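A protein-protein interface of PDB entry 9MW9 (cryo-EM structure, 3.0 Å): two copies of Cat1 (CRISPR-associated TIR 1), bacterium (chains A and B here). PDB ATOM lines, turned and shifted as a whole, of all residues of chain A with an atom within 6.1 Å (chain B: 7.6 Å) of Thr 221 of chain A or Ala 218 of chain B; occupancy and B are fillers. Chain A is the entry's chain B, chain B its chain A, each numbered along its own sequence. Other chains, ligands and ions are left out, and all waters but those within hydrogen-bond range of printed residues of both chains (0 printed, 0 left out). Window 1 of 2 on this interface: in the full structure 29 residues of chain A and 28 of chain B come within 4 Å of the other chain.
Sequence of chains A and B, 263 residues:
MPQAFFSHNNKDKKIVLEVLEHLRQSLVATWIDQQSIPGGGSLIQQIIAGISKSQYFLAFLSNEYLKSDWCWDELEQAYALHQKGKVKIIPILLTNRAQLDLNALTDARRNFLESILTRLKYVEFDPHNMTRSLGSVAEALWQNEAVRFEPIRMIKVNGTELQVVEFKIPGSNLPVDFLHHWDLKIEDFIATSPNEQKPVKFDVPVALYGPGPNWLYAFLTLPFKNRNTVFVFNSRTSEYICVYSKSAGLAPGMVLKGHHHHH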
ATOM      1  N   LEU A 208       4.701  15.606  23.532  1.00  0.00           N
ATOM      2  CA  LEU A 208       4.917  15.430  24.962  1.00  0.00           C
ATOM      3  C   LEU A 208       4.919  13.945  25.292  1.00  0.00           C
ATOM      4  O   LEU A 208       3.977  13.225  24.942  1.00  0.00           O
ATOM      5  CB  LEU A 208       3.844  16.156  25.773  1.00  0.00           C
ATOM      6  CG  LEU A 208       4.117  17.621  26.122  1.00  0.00           C
ATOM      7  CD1 LEU A 208       5.488  17.771  26.757  1.00  0.00           C
ATOM      8  CD2 LEU A 208       3.990  18.513  24.896  1.00  0.00           C
ATOM      9  N   LEU A 216      -0.037  18.724  34.747  1.00  0.00           N
ATOM     10  CA  LEU A 216       1.309  18.917  34.219  1.00  0.00           C
ATOM     11  C   LEU A 216       1.296  19.003  32.699  1.00  0.00           C
ATOM     12  O   LEU A 216       1.989  19.841  32.113  1.00  0.00           O
ATOM     13  CB  LEU A 216       2.227  17.788  34.681  1.00  0.00           C
ATOM     14  CG  LEU A 216       3.683  17.902  34.235  1.00  0.00           C
ATOM     15  CD1 LEU A 216       4.246  19.264  34.597  1.00  0.00           C
ATOM     16  CD2 LEU A 216       4.517  16.797  34.852  1.00  0.00           C
ATOM     17  N   TYR A 217       0.517  18.139  32.045  1.00  0.00           N
ATOM     18  CA  TYR A 217       0.394  18.210  30.593  1.00  0.00           C
ATOM     19  C   TYR A 217      -0.240  19.523  30.157  1.00  0.00           C
ATOM     20  O   TYR A 217       0.258  20.187  29.241  1.00  0.00           O
ATOM     21  CB  TYR A 217      -0.419  17.027  30.076  1.00  0.00           C
ATOM     22  CG  TYR A 217       0.415  15.821  29.730  1.00  0.00           C
ATOM     23  CD1 TYR A 217       1.776  15.800  29.983  1.00  0.00           C
ATOM     24  CD2 TYR A 217      -0.158  14.703  29.148  1.00  0.00           C
ATOM     25  CE1 TYR A 217       2.541  14.701  29.666  1.00  0.00           C
ATOM     26  CE2 TYR A 217       0.601  13.597  28.830  1.00  0.00           C
ATOM     27  CZ  TYR A 217       1.950  13.602  29.091  1.00  0.00           C
ATOM     28  OH  TYR A 217       2.714  12.502  28.775  1.00  0.00           O
ATOM     29  N   ALA A 218      -1.335  19.919  30.809  1.00  0.00           N
ATOM     30  CA  ALA A 218      -2.004  21.161  30.438  1.00  0.00           C
ATOM     31  C   ALA A 218      -1.089  22.360  30.637  1.00  0.00           C
ATOM     32  O   ALA A 218      -1.170  23.344  29.893  1.00  0.00           O
ATOM     33  CB  ALA A 218      -3.291  21.326  31.245  1.00  0.00           C
ATOM     34  N   PHE A 219      -0.210  22.298  31.638  1.00  0.00           N
ATOM     35  CA  PHE A 219       0.720  23.396  31.873  1.00  0.00           C
ATOM     36  C   PHE A 219       1.739  23.515  30.747  1.00  0.00           C
ATOM     37  O   PHE A 219       2.137  24.625  30.377  1.00  0.00           O
ATOM     38  CB  PHE A 219       1.427  23.206  33.213  1.00  0.00           C
ATOM     39  CG  PHE A 219       2.556  24.166  33.444  1.00  0.00           C
ATOM     40  CD1 PHE A 219       2.303  25.489  33.760  1.00  0.00           C
ATOM     41  CD2 PHE A 219       3.871  23.746  33.346  1.00  0.00           C
ATOM     42  CE1 PHE A 219       3.340  26.374  33.975  1.00  0.00           C
ATOM     43  CE2 PHE A 219       4.912  24.627  33.558  1.00  0.00           C
ATOM     44  CZ  PHE A 219       4.645  25.943  33.873  1.00  0.00           C
ATOM     45  N   LEU A 220       2.176  22.384  30.193  1.00  0.00           N
ATOM     46  CA  LEU A 220       3.256  22.410  29.212  1.00  0.00           C
ATOM     47  C   LEU A 220       2.766  22.806  27.823  1.00  0.00           C
ATOM     48  O   LEU A 220       3.410  23.613  27.145  1.00  0.00           O
ATOM     49  CB  LEU A 220       3.947  21.049  29.162  1.00  0.00           C
ATOM     50  CG  LEU A 220       4.847  20.716  30.353  1.00  0.00           C
ATOM     51  CD1 LEU A 220       5.734  19.524  30.039  1.00  0.00           C
ATOM     52  CD2 LEU A 220       5.686  21.920  30.743  1.00  0.00           C
ATOM     53  N   THR A 221       1.637  22.249  27.379  1.00  0.00           N
ATOM     54  CA  THR A 221       1.185  22.506  26.017  1.00  0.00           C
ATOM     55  C   THR A 221       0.544  23.882  25.880  1.00  0.00           C
ATOM     56  O   THR A 221       0.453  24.418  24.771  1.00  0.00           O
ATOM     57  CB  THR A 221       0.206  21.422  25.568  1.00  0.00           C
ATOM     58  OG1 THR A 221      -1.121  21.769  25.984  1.00  0.00           O
ATOM     59  CG2 THR A 221       0.591  20.075  26.151  1.00  0.00           C
ATOM     60  N   LEU A 222       0.092  24.464  26.990  1.00  0.00           N
ATOM     61  CA  LEU A 222      -0.646  25.725  26.914  1.00  0.00           C
ATOM     62  C   LEU A 222       0.153  26.864  26.293  1.00  0.00           C
ATOM     63  O   LEU A 222      -0.383  27.545  25.402  1.00  0.00           O
ATOM     64  CB  LEU A 222      -1.164  26.102  28.305  1.00  0.00           C
ATOM     65  CG  LEU A 222      -2.201  27.224  28.372  1.00  0.00           C
ATOM     66  CD1 LEU A 222      -3.131  27.185  27.177  1.00  0.00           C
ATOM     67  CD2 LEU A 222      -2.995  27.099  29.649  1.00  0.00           C
ATOM     68  N   PRO A 223       1.404  27.137  26.685  1.00  0.00           N
ATOM     69  CA  PRO A 223       2.118  28.273  26.083  1.00  0.00           C
ATOM     70  C   PRO A 223       2.539  28.053  24.641  1.00  0.00           C
ATOM     71  O   PRO A 223       3.252  28.899  24.091  1.00  0.00           O
ATOM     72  CB  PRO A 223       3.346  28.437  26.993  1.00  0.00           C
ATOM     73  CG  PRO A 223       3.014  27.693  28.240  1.00  0.00           C
ATOM     74  CD  PRO A 223       2.188  26.545  27.781  1.00  0.00           C
ATOM     75  N   PHE A 224       2.132  26.956  24.009  1.00  0.00           N
ATOM     76  CA  PHE A 224       2.481  26.686  22.622  1.00  0.00           C
ATOM     77  C   PHE A 224       1.433  27.176  21.634  1.00  0.00           C
ATOM     78  O   PHE A 224       1.587  26.948  20.430  1.00  0.00           O
ATOM     79  CB  PHE A 224       2.707  25.188  22.416  1.00  0.00           C
ATOM     80  CG  PHE A 224       4.085  24.728  22.782  1.00  0.00           C
ATOM     81  CD1 PHE A 224       5.180  25.114  22.031  1.00  0.00           C
ATOM     82  CD2 PHE A 224       4.286  23.902  23.873  1.00  0.00           C
ATOM     83  CE1 PHE A 224       6.450  24.689  22.364  1.00  0.00           C
ATOM     84  CE2 PHE A 224       5.553  23.474  24.211  1.00  0.00           C
ATOM     85  CZ  PHE A 224       6.636  23.868  23.455  1.00  0.00           C
ATOM     86  N   LYS A 225       0.372  27.827  22.105  1.00  0.00           N
ATOM     87  CA  LYS A 225      -0.653  28.338  21.203  1.00  0.00           C
ATOM     88  C   LYS A 225      -0.059  29.396  20.285  1.00  0.00           C
ATOM     89  O   LYS A 225       0.694  30.267  20.730  1.00  0.00           O
ATOM     90  CB  LYS A 225      -1.821  28.915  21.999  1.00  0.00           C
ATOM     91  CG  LYS A 225      -2.995  29.353  21.140  1.00  0.00           C
ATOM     92  CD  LYS A 225      -4.075  30.016  21.978  1.00  0.00           C
ATOM     93  CE  LYS A 225      -5.167  30.608  21.104  1.00  0.00           C
ATOM     94  NZ  LYS A 225      -6.144  31.400  21.899  1.00  0.00           N
ATOM     95  N   VAL A 230       1.128  20.879  18.728  1.00  0.00           N
ATOM     96  CA  VAL A 230       1.423  20.097  19.923  1.00  0.00           C
ATOM     97  C   VAL A 230       0.859  18.695  19.763  1.00  0.00           C
ATOM     98  O   VAL A 230      -0.320  18.522  19.428  1.00  0.00           O
ATOM     99  CB  VAL A 230       0.860  20.774  21.183  1.00  0.00           C
ATOM    100  CG1 VAL A 230       0.744  19.771  22.316  1.00  0.00           C
ATOM    101  CG2 VAL A 230       1.745  21.925  21.592  1.00  0.00           C
ATOM    102  N   PHE A 231       1.701  17.695  20.002  1.00  0.00           N
ATOM    103  CA  PHE A 231       1.291  16.303  20.069  1.00  0.00           C
ATOM    104  C   PHE A 231       1.452  15.804  21.497  1.00  0.00           C
ATOM    105  O   PHE A 231       2.303  16.287  22.248  1.00  0.00           O
ATOM    106  CB  PHE A 231       2.114  15.429  19.119  1.00  0.00           C
ATOM    107  CG  PHE A 231       1.561  15.359  17.727  1.00  0.00           C
ATOM    108  CD1 PHE A 231       1.843  16.349  16.804  1.00  0.00           C
ATOM    109  CD2 PHE A 231       0.764  14.297  17.340  1.00  0.00           C
ATOM    110  CE1 PHE A 231       1.338  16.283  15.522  1.00  0.00           C
ATOM    111  CE2 PHE A 231       0.256  14.225  16.060  1.00  0.00           C
ATOM    112  CZ  PHE A 231       0.544  15.220  15.151  1.00  0.00           C
ATOM    113  N   VAL A 232       0.618  14.841  21.875  1.00  0.00           N
ATOM    114  CA  VAL A 232       0.687  14.232  23.195  1.00  0.00           C
ATOM    115  C   VAL A 232       0.624  12.722  23.041  1.00  0.00           C
ATOM    116  O   VAL A 232       0.027  12.198  22.097  1.00  0.00           O
ATOM    117  CB  VAL A 232      -0.439  14.734  24.123  1.00  0.00           C
ATOM    118  CG1 VAL A 232      -0.076  16.086  24.706  1.00  0.00           C
ATOM    119  CG2 VAL A 232      -1.738  14.820  23.359  1.00  0.00           C
ATOM    120  N   VAL A 243      -3.389  17.683  19.259  1.00  0.00           N
ATOM    121  CA  VAL A 243      -4.355  18.522  19.957  1.00  0.00           C
ATOM    122  C   VAL A 243      -4.332  19.967  19.489  1.00  0.00           C
ATOM    123  O   VAL A 243      -5.257  20.724  19.826  1.00  0.00           O
ATOM    124  CB  VAL A 243      -4.152  18.463  21.485  1.00  0.00           C
ATOM    125  CG1 VAL A 243      -4.485  17.076  22.011  1.00  0.00           C
ATOM    126  CG2 VAL A 243      -2.734  18.846  21.839  1.00  0.00           C
ATOM    127  N   LEU B 179     -11.051  13.151  18.280  1.00  0.00           N
ATOM    128  CA  LEU B 179     -10.897  14.593  18.123  1.00  0.00           C
ATOM    129  C   LEU B 179     -11.000  15.033  16.671  1.00  0.00           C
ATOM    130  O   LEU B 179     -11.297  16.204  16.409  1.00  0.00           O
ATOM    131  CB  LEU B 179      -9.557  15.040  18.706  1.00  0.00           C
ATOM    132  CG  LEU B 179      -9.577  15.527  20.154  1.00  0.00           C
ATOM    133  CD1 LEU B 179      -8.281  16.240  20.489  1.00  0.00           C
ATOM    134  CD2 LEU B 179     -10.770  16.432  20.396  1.00  0.00           C
ATOM    135  N   LEU B 208     -11.694  23.007  34.535  1.00  0.00           N
ATOM    136  CA  LEU B 208     -12.060  21.789  33.825  1.00  0.00           C
ATOM    137  C   LEU B 208     -12.165  20.654  34.832  1.00  0.00           C
ATOM    138  O   LEU B 208     -11.233  20.422  35.609  1.00  0.00           O
ATOM    139  CB  LEU B 208     -11.036  21.458  32.740  1.00  0.00           C
ATOM    140  CG  LEU B 208     -11.131  22.298  31.468  1.00  0.00           C
ATOM    141  CD1 LEU B 208      -9.968  21.995  30.543  1.00  0.00           C
ATOM    142  CD2 LEU B 208     -12.454  22.050  30.767  1.00  0.00           C
ATOM    143  N   PRO B 213      -8.995  11.433  29.198  1.00  0.00           N
ATOM    144  CA  PRO B 213      -7.613  11.225  28.759  1.00  0.00           C
ATOM    145  C   PRO B 213      -6.820  12.521  28.793  1.00  0.00           C
ATOM    146  O   PRO B 213      -7.362  13.623  28.902  1.00  0.00           O
ATOM    147  CB  PRO B 213      -7.771  10.702  27.330  1.00  0.00           C
ATOM    148  CG  PRO B 213      -9.061  11.274  26.873  1.00  0.00           C
ATOM    149  CD  PRO B 213      -9.951  11.342  28.082  1.00  0.00           C
ATOM    150  N   ASN B 214      -5.498  12.367  28.704  1.00  0.00           N
ATOM    151  CA  ASN B 214      -4.608  13.522  28.754  1.00  0.00           C
ATOM    152  C   ASN B 214      -4.845  14.461  27.578  1.00  0.00           C
ATOM    153  O   ASN B 214      -4.866  15.686  27.749  1.00  0.00           O
ATOM    154  CB  ASN B 214      -3.155  13.054  28.780  1.00  0.00           C
ATOM    155  CG  ASN B 214      -2.844  12.067  27.675  1.00  0.00           C
ATOM    156  OD1 ASN B 214      -3.748  11.472  27.091  1.00  0.00           O
ATOM    157  ND2 ASN B 214      -1.564  11.887  27.381  1.00  0.00           N
ATOM    158  N   TRP B 215      -5.024  13.910  26.376  1.00  0.00           N
ATOM    159  CA  TRP B 215      -5.189  14.759  25.200  1.00  0.00           C
ATOM    160  C   TRP B 215      -6.496  15.537  25.243  1.00  0.00           C
ATOM    161  O   TRP B 215      -6.559  16.661  24.734  1.00  0.00           O
ATOM    162  CB  TRP B 215      -5.105  13.927  23.920  1.00  0.00           C
ATOM    163  CG  TRP B 215      -5.820  12.618  23.973  1.00  0.00           C
ATOM    164  CD1 TRP B 215      -5.325  11.433  24.428  1.00  0.00           C
ATOM    165  CD2 TRP B 215      -7.155  12.352  23.530  1.00  0.00           C
ATOM    166  NE1 TRP B 215      -6.272  10.448  24.309  1.00  0.00           N
ATOM    167  CE2 TRP B 215      -7.405  10.986  23.758  1.00  0.00           C
ATOM    168  CE3 TRP B 215      -8.164  13.138  22.968  1.00  0.00           C
ATOM    169  CZ2 TRP B 215      -8.621  10.390  23.444  1.00  0.00           C
ATOM    170  CZ3 TRP B 215      -9.371  12.542  22.657  1.00  0.00           C
ATOM    171  CH2 TRP B 215      -9.590  11.183  22.896  1.00  0.00           C
ATOM    172  N   LEU B 216      -7.546  14.962  25.832  1.00  0.00           N
ATOM    173  CA  LEU B 216      -8.803  15.690  25.955  1.00  0.00           C
ATOM    174  C   LEU B 216      -8.639  16.927  26.826  1.00  0.00           C
ATOM    175  O   LEU B 216      -9.179  17.994  26.511  1.00  0.00           O
ATOM    176  CB  LEU B 216      -9.889  14.779  26.521  1.00  0.00           C
ATOM    177  CG  LEU B 216     -11.315  15.307  26.381  1.00  0.00           C
ATOM    178  CD1 LEU B 216     -11.675  15.471  24.917  1.00  0.00           C
ATOM    179  CD2 LEU B 216     -12.293  14.378  27.072  1.00  0.00           C
ATOM    180  N   TYR B 217      -7.903  16.804  27.933  1.00  0.00           N
ATOM    181  CA  TYR B 217      -7.651  17.966  28.778  1.00  0.00           C
ATOM    182  C   TYR B 217      -6.806  19.004  28.052  1.00  0.00           C
ATOM    183  O   TYR B 217      -7.080  20.206  28.138  1.00  0.00           O
ATOM    184  CB  TYR B 217      -6.976  17.534  30.078  1.00  0.00           C
ATOM    185  CG  TYR B 217      -7.955  17.250  31.188  1.00  0.00           C
ATOM    186  CD1 TYR B 217      -8.567  16.012  31.301  1.00  0.00           C
ATOM    187  CD2 TYR B 217      -8.281  18.229  32.117  1.00  0.00           C
ATOM    188  CE1 TYR B 217      -9.468  15.752  32.312  1.00  0.00           C
ATOM    189  CE2 TYR B 217      -9.179  17.979  33.128  1.00  0.00           C
ATOM    190  CZ  TYR B 217      -9.769  16.740  33.222  1.00  0.00           C
ATOM    191  OH  TYR B 217     -10.667  16.490  34.231  1.00  0.00           O
ATOM    192  N   ALA B 218      -5.774  18.560  27.333  1.00  0.00           N
ATOM    193  CA  ALA B 218      -4.930  19.495  26.597  1.00  0.00           C
ATOM    194  C   ALA B 218      -5.711  20.194  25.493  1.00  0.00           C
ATOM    195  O   ALA B 218      -5.538  21.399  25.270  1.00  0.00           O
ATOM    196  CB  ALA B 218      -3.719  18.767  26.020  1.00  0.00           C
ATOM    197  N   PHE B 219      -6.572  19.457  24.790  1.00  0.00           N
ATOM    198  CA  PHE B 219      -7.330  20.048  23.691  1.00  0.00           C
ATOM    199  C   PHE B 219      -8.294  21.115  24.191  1.00  0.00           C
ATOM    200  O   PHE B 219      -8.483  22.143  23.532  1.00  0.00           O
ATOM    201  CB  PHE B 219      -8.080  18.957  22.930  1.00  0.00           C
ATOM    202  CG  PHE B 219      -9.039  19.484  21.905  1.00  0.00           C
ATOM    203  CD1 PHE B 219      -8.581  19.953  20.687  1.00  0.00           C
ATOM    204  CD2 PHE B 219     -10.399  19.499  22.152  1.00  0.00           C
ATOM    205  CE1 PHE B 219      -9.460  20.435  19.740  1.00  0.00           C
ATOM    206  CE2 PHE B 219     -11.284  19.980  21.208  1.00  0.00           C
ATOM    207  CZ  PHE B 219     -10.814  20.448  20.001  1.00  0.00           C
ATOM    208  N   LEU B 220      -8.926  20.885  25.343  1.00  0.00           N
ATOM    209  CA  LEU B 220      -9.834  21.886  25.899  1.00  0.00           C
ATOM    210  C   LEU B 220      -9.069  23.063  26.490  1.00  0.00           C
ATOM    211  O   LEU B 220      -9.502  24.215  26.370  1.00  0.00           O
ATOM    212  CB  LEU B 220     -10.732  21.249  26.960  1.00  0.00           C
ATOM    213  CG  LEU B 220     -11.695  20.128  26.563  1.00  0.00           C
ATOM    214  CD1 LEU B 220     -12.933  20.172  27.439  1.00  0.00           C
ATOM    215  CD2 LEU B 220     -12.091  20.238  25.105  1.00  0.00           C
ATOM    216  N   THR B 221      -7.931  22.794  27.132  1.00  0.00           N
ATOM    217  CA  THR B 221      -7.214  23.844  27.851  1.00  0.00           C
ATOM    218  C   THR B 221      -6.503  24.795  26.895  1.00  0.00           C
ATOM    219  O   THR B 221      -6.481  26.010  27.123  1.00  0.00           O
ATOM    220  CB  THR B 221      -6.219  23.211  28.826  1.00  0.00           C
ATOM    221  OG1 THR B 221      -6.903  22.823  30.022  1.00  0.00           O
ATOM    222  CG2 THR B 221      -5.106  24.180  29.182  1.00  0.00           C
ATOM    223  N   LEU B 222      -5.935  24.263  25.814  1.00  0.00           N
ATOM    224  CA  LEU B 222      -5.037  25.050  24.969  1.00  0.00           C
ATOM    225  C   LEU B 222      -5.660  26.320  24.399  1.00  0.00           C
ATOM    226  O   LEU B 222      -5.017  27.380  24.480  1.00  0.00           O
ATOM    227  CB  LEU B 222      -4.480  24.158  23.857  1.00  0.00           C
ATOM    228  CG  LEU B 222      -3.425  24.793  22.957  1.00  0.00           C
ATOM    229  CD1 LEU B 222      -2.388  25.525  23.775  1.00  0.00           C
ATOM    230  CD2 LEU B 222      -2.764  23.715  22.142  1.00  0.00           C
ATOM    231  N   PRO B 223      -6.867  26.309  23.820  1.00  0.00           N
ATOM    232  CA  PRO B 223      -7.387  27.542  23.209  1.00  0.00           C
ATOM    233  C   PRO B 223      -7.683  28.657  24.199  1.00  0.00           C
ATOM    234  O   PRO B 223      -8.075  29.747  23.770  1.00  0.00           O
ATOM    235  CB  PRO B 223      -8.676  27.074  22.516  1.00  0.00           C
ATOM    236  CG  PRO B 223      -8.516  25.607  22.361  1.00  0.00           C
ATOM    237  CD  PRO B 223      -7.778  25.178  23.580  1.00  0.00           C
ATOM    238  N   PHE B 224      -7.511  28.431  25.497  1.00  0.00           N
ATOM    239  CA  PHE B 224      -7.813  29.439  26.502  1.00  0.00           C
ATOM    240  C   PHE B 224      -6.648  30.379  26.777  1.00  0.00           C
ATOM    241  O   PHE B 224      -6.780  31.266  27.627  1.00  0.00           O
ATOM    242  CB  PHE B 224      -8.241  28.768  27.806  1.00  0.00           C
ATOM    243  CG  PHE B 224      -9.700  28.437  27.864  1.00  0.00           C
ATOM    244  CD1 PHE B 224     -10.653  29.432  27.752  1.00  0.00           C
ATOM    245  CD2 PHE B 224     -10.120  27.130  28.026  1.00  0.00           C
ATOM    246  CE1 PHE B 224     -11.997  29.130  27.803  1.00  0.00           C
ATOM    247  CE2 PHE B 224     -11.462  26.821  28.078  1.00  0.00           C
ATOM    248  CZ  PHE B 224     -12.402  27.823  27.966  1.00  0.00           C
ATOM    249  N   LYS B 225      -5.519  30.205  26.097  1.00  0.00           N
ATOM    250  CA  LYS B 225      -4.394  31.109  26.284  1.00  0.00           C
ATOM    251  C   LYS B 225      -4.776  32.518  25.852  1.00  0.00           C
ATOM    252  O   LYS B 225      -5.490  32.709  24.863  1.00  0.00           O
ATOM    253  CB  LYS B 225      -3.181  30.625  25.492  1.00  0.00           C
ATOM    254  CG  LYS B 225      -1.903  31.388  25.790  1.00  0.00           C
ATOM    255  CD  LYS B 225      -0.791  30.994  24.837  1.00  0.00           C
ATOM    256  CE  LYS B 225       0.475  31.783  25.110  1.00  0.00           C
ATOM    257  NZ  LYS B 225       1.496  31.568  24.049  1.00  0.00           N
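Ala 218 of chain A touches Thr 221 of chain B, and with the chains exchanged Thr 221 of chain A touches Ala 218 of chain B.
Thr 221 of chain A touches Leu 222 of chain B, and with the chains exchanged Leu 222 of chain A touches Thr 221 of chain B.
Leu 222 of chain B touches its own counterpart, Leu 222 of chain A.
Pro 223 of chain A touches Lys 225 of chain B, and with the chains exchanged Lys 225 of chain A touches Pro 223 of chain B.
Positions printed for both chains: 208, 216, 217, 218, 219, 220, 221, 222, 223, 224 and 225.
Phe 219 of chain A touches none of the printed residues of chain B.
Leu 220 of chain A touches none of the printed residues of chain B.
Of chain B, only Ala 218 (3.97 Å) and Leu 222 (3.2 Å) come within 4 Å of Thr 221 of chain A.
Printed residues of chain B within 4 Å of Val 232 of chain A: Trp 215 (3.5 Å).
Of the printed residues of chain A, Asn 214 of chain B touches Tyr 217 (3.1 Å).
Printed residues of chain A within 4 Å of Ala 218 of chain B: Thr 221.
Of the printed residues of chain A, Thr 221 of chain B touches Ala 218 (3.96 Å) and Leu 222 (3.6 Å).
The nearest residue of chain B that does not touch Thr 221 of chain A is Thr 221 of chain B (5.6 Å).
The nearest residue of chain A that does not touch Ala 218 of chain B is Val 243 of chain A (4.3 Å).
Among the printed residues, merely in contact across the chains: Tyr 217 of chain A with Asn 214 of chain B, Thr 221 of chain A with Leu 222 of chain B, Leu 222 of chain A with Leu 222 of chain B, Val 243 of chain A with Trp 215 of chain B, Leu 222 of chain A with Lys 225 of chain B, Val 243 of chain A with Phe 219 of chain B, Val 232 of chain A with Trp 215 of chain B, Leu 222 of chain A with Thr 221 of chain B, Lys 225 of chain A with Leu 222 of chain B, Ala 218 of chain A with Thr 221 of chain B and Thr 221 of chain A with Ala 218 of chain B.
O of Pro 223 of chain B is in hydrogen-bond range of NZ of Lys 225 of chain A (3.2 Å).
The backbone carbonyl oxygen (O) of Pro 223 of chain A lies within hydrogen-bond range of the side-chain amino group (NZ) of Lys 225 of chain B, 3.2 Å away.
O of Lys 225 of chain B is in hydrogen-bond range of NZ of Lys 225 of chain A, at 3.3 Å.
Of the 15 printed residues of chain A, 8 touch a printed residue of chain B.
Along chain A the printed residues that touch a printed residue of chain B span positions 217 to 243.
Hydrophobic or aromatic side chains of chain B that line the printed part of chain A: Trp 215, Ala 218, Phe 219 and Leu 222.
Among the printed residues, 14 pairs touch across the chains.
Among the printed residues, no Asp or Glu carboxylate lies within 4 Å of a Lys or Arg side-chain nitrogen of the other chain.
O of Tyr 217 of chain B lies close to OG1 of Thr 221 of chain B (3.2 Å).
The backbone carbonyl oxygen (O) of Val 230 of chain A sits at hydrogen-bond distance from the backbone NH (N) of Val 243 of chain A (3.2 Å).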
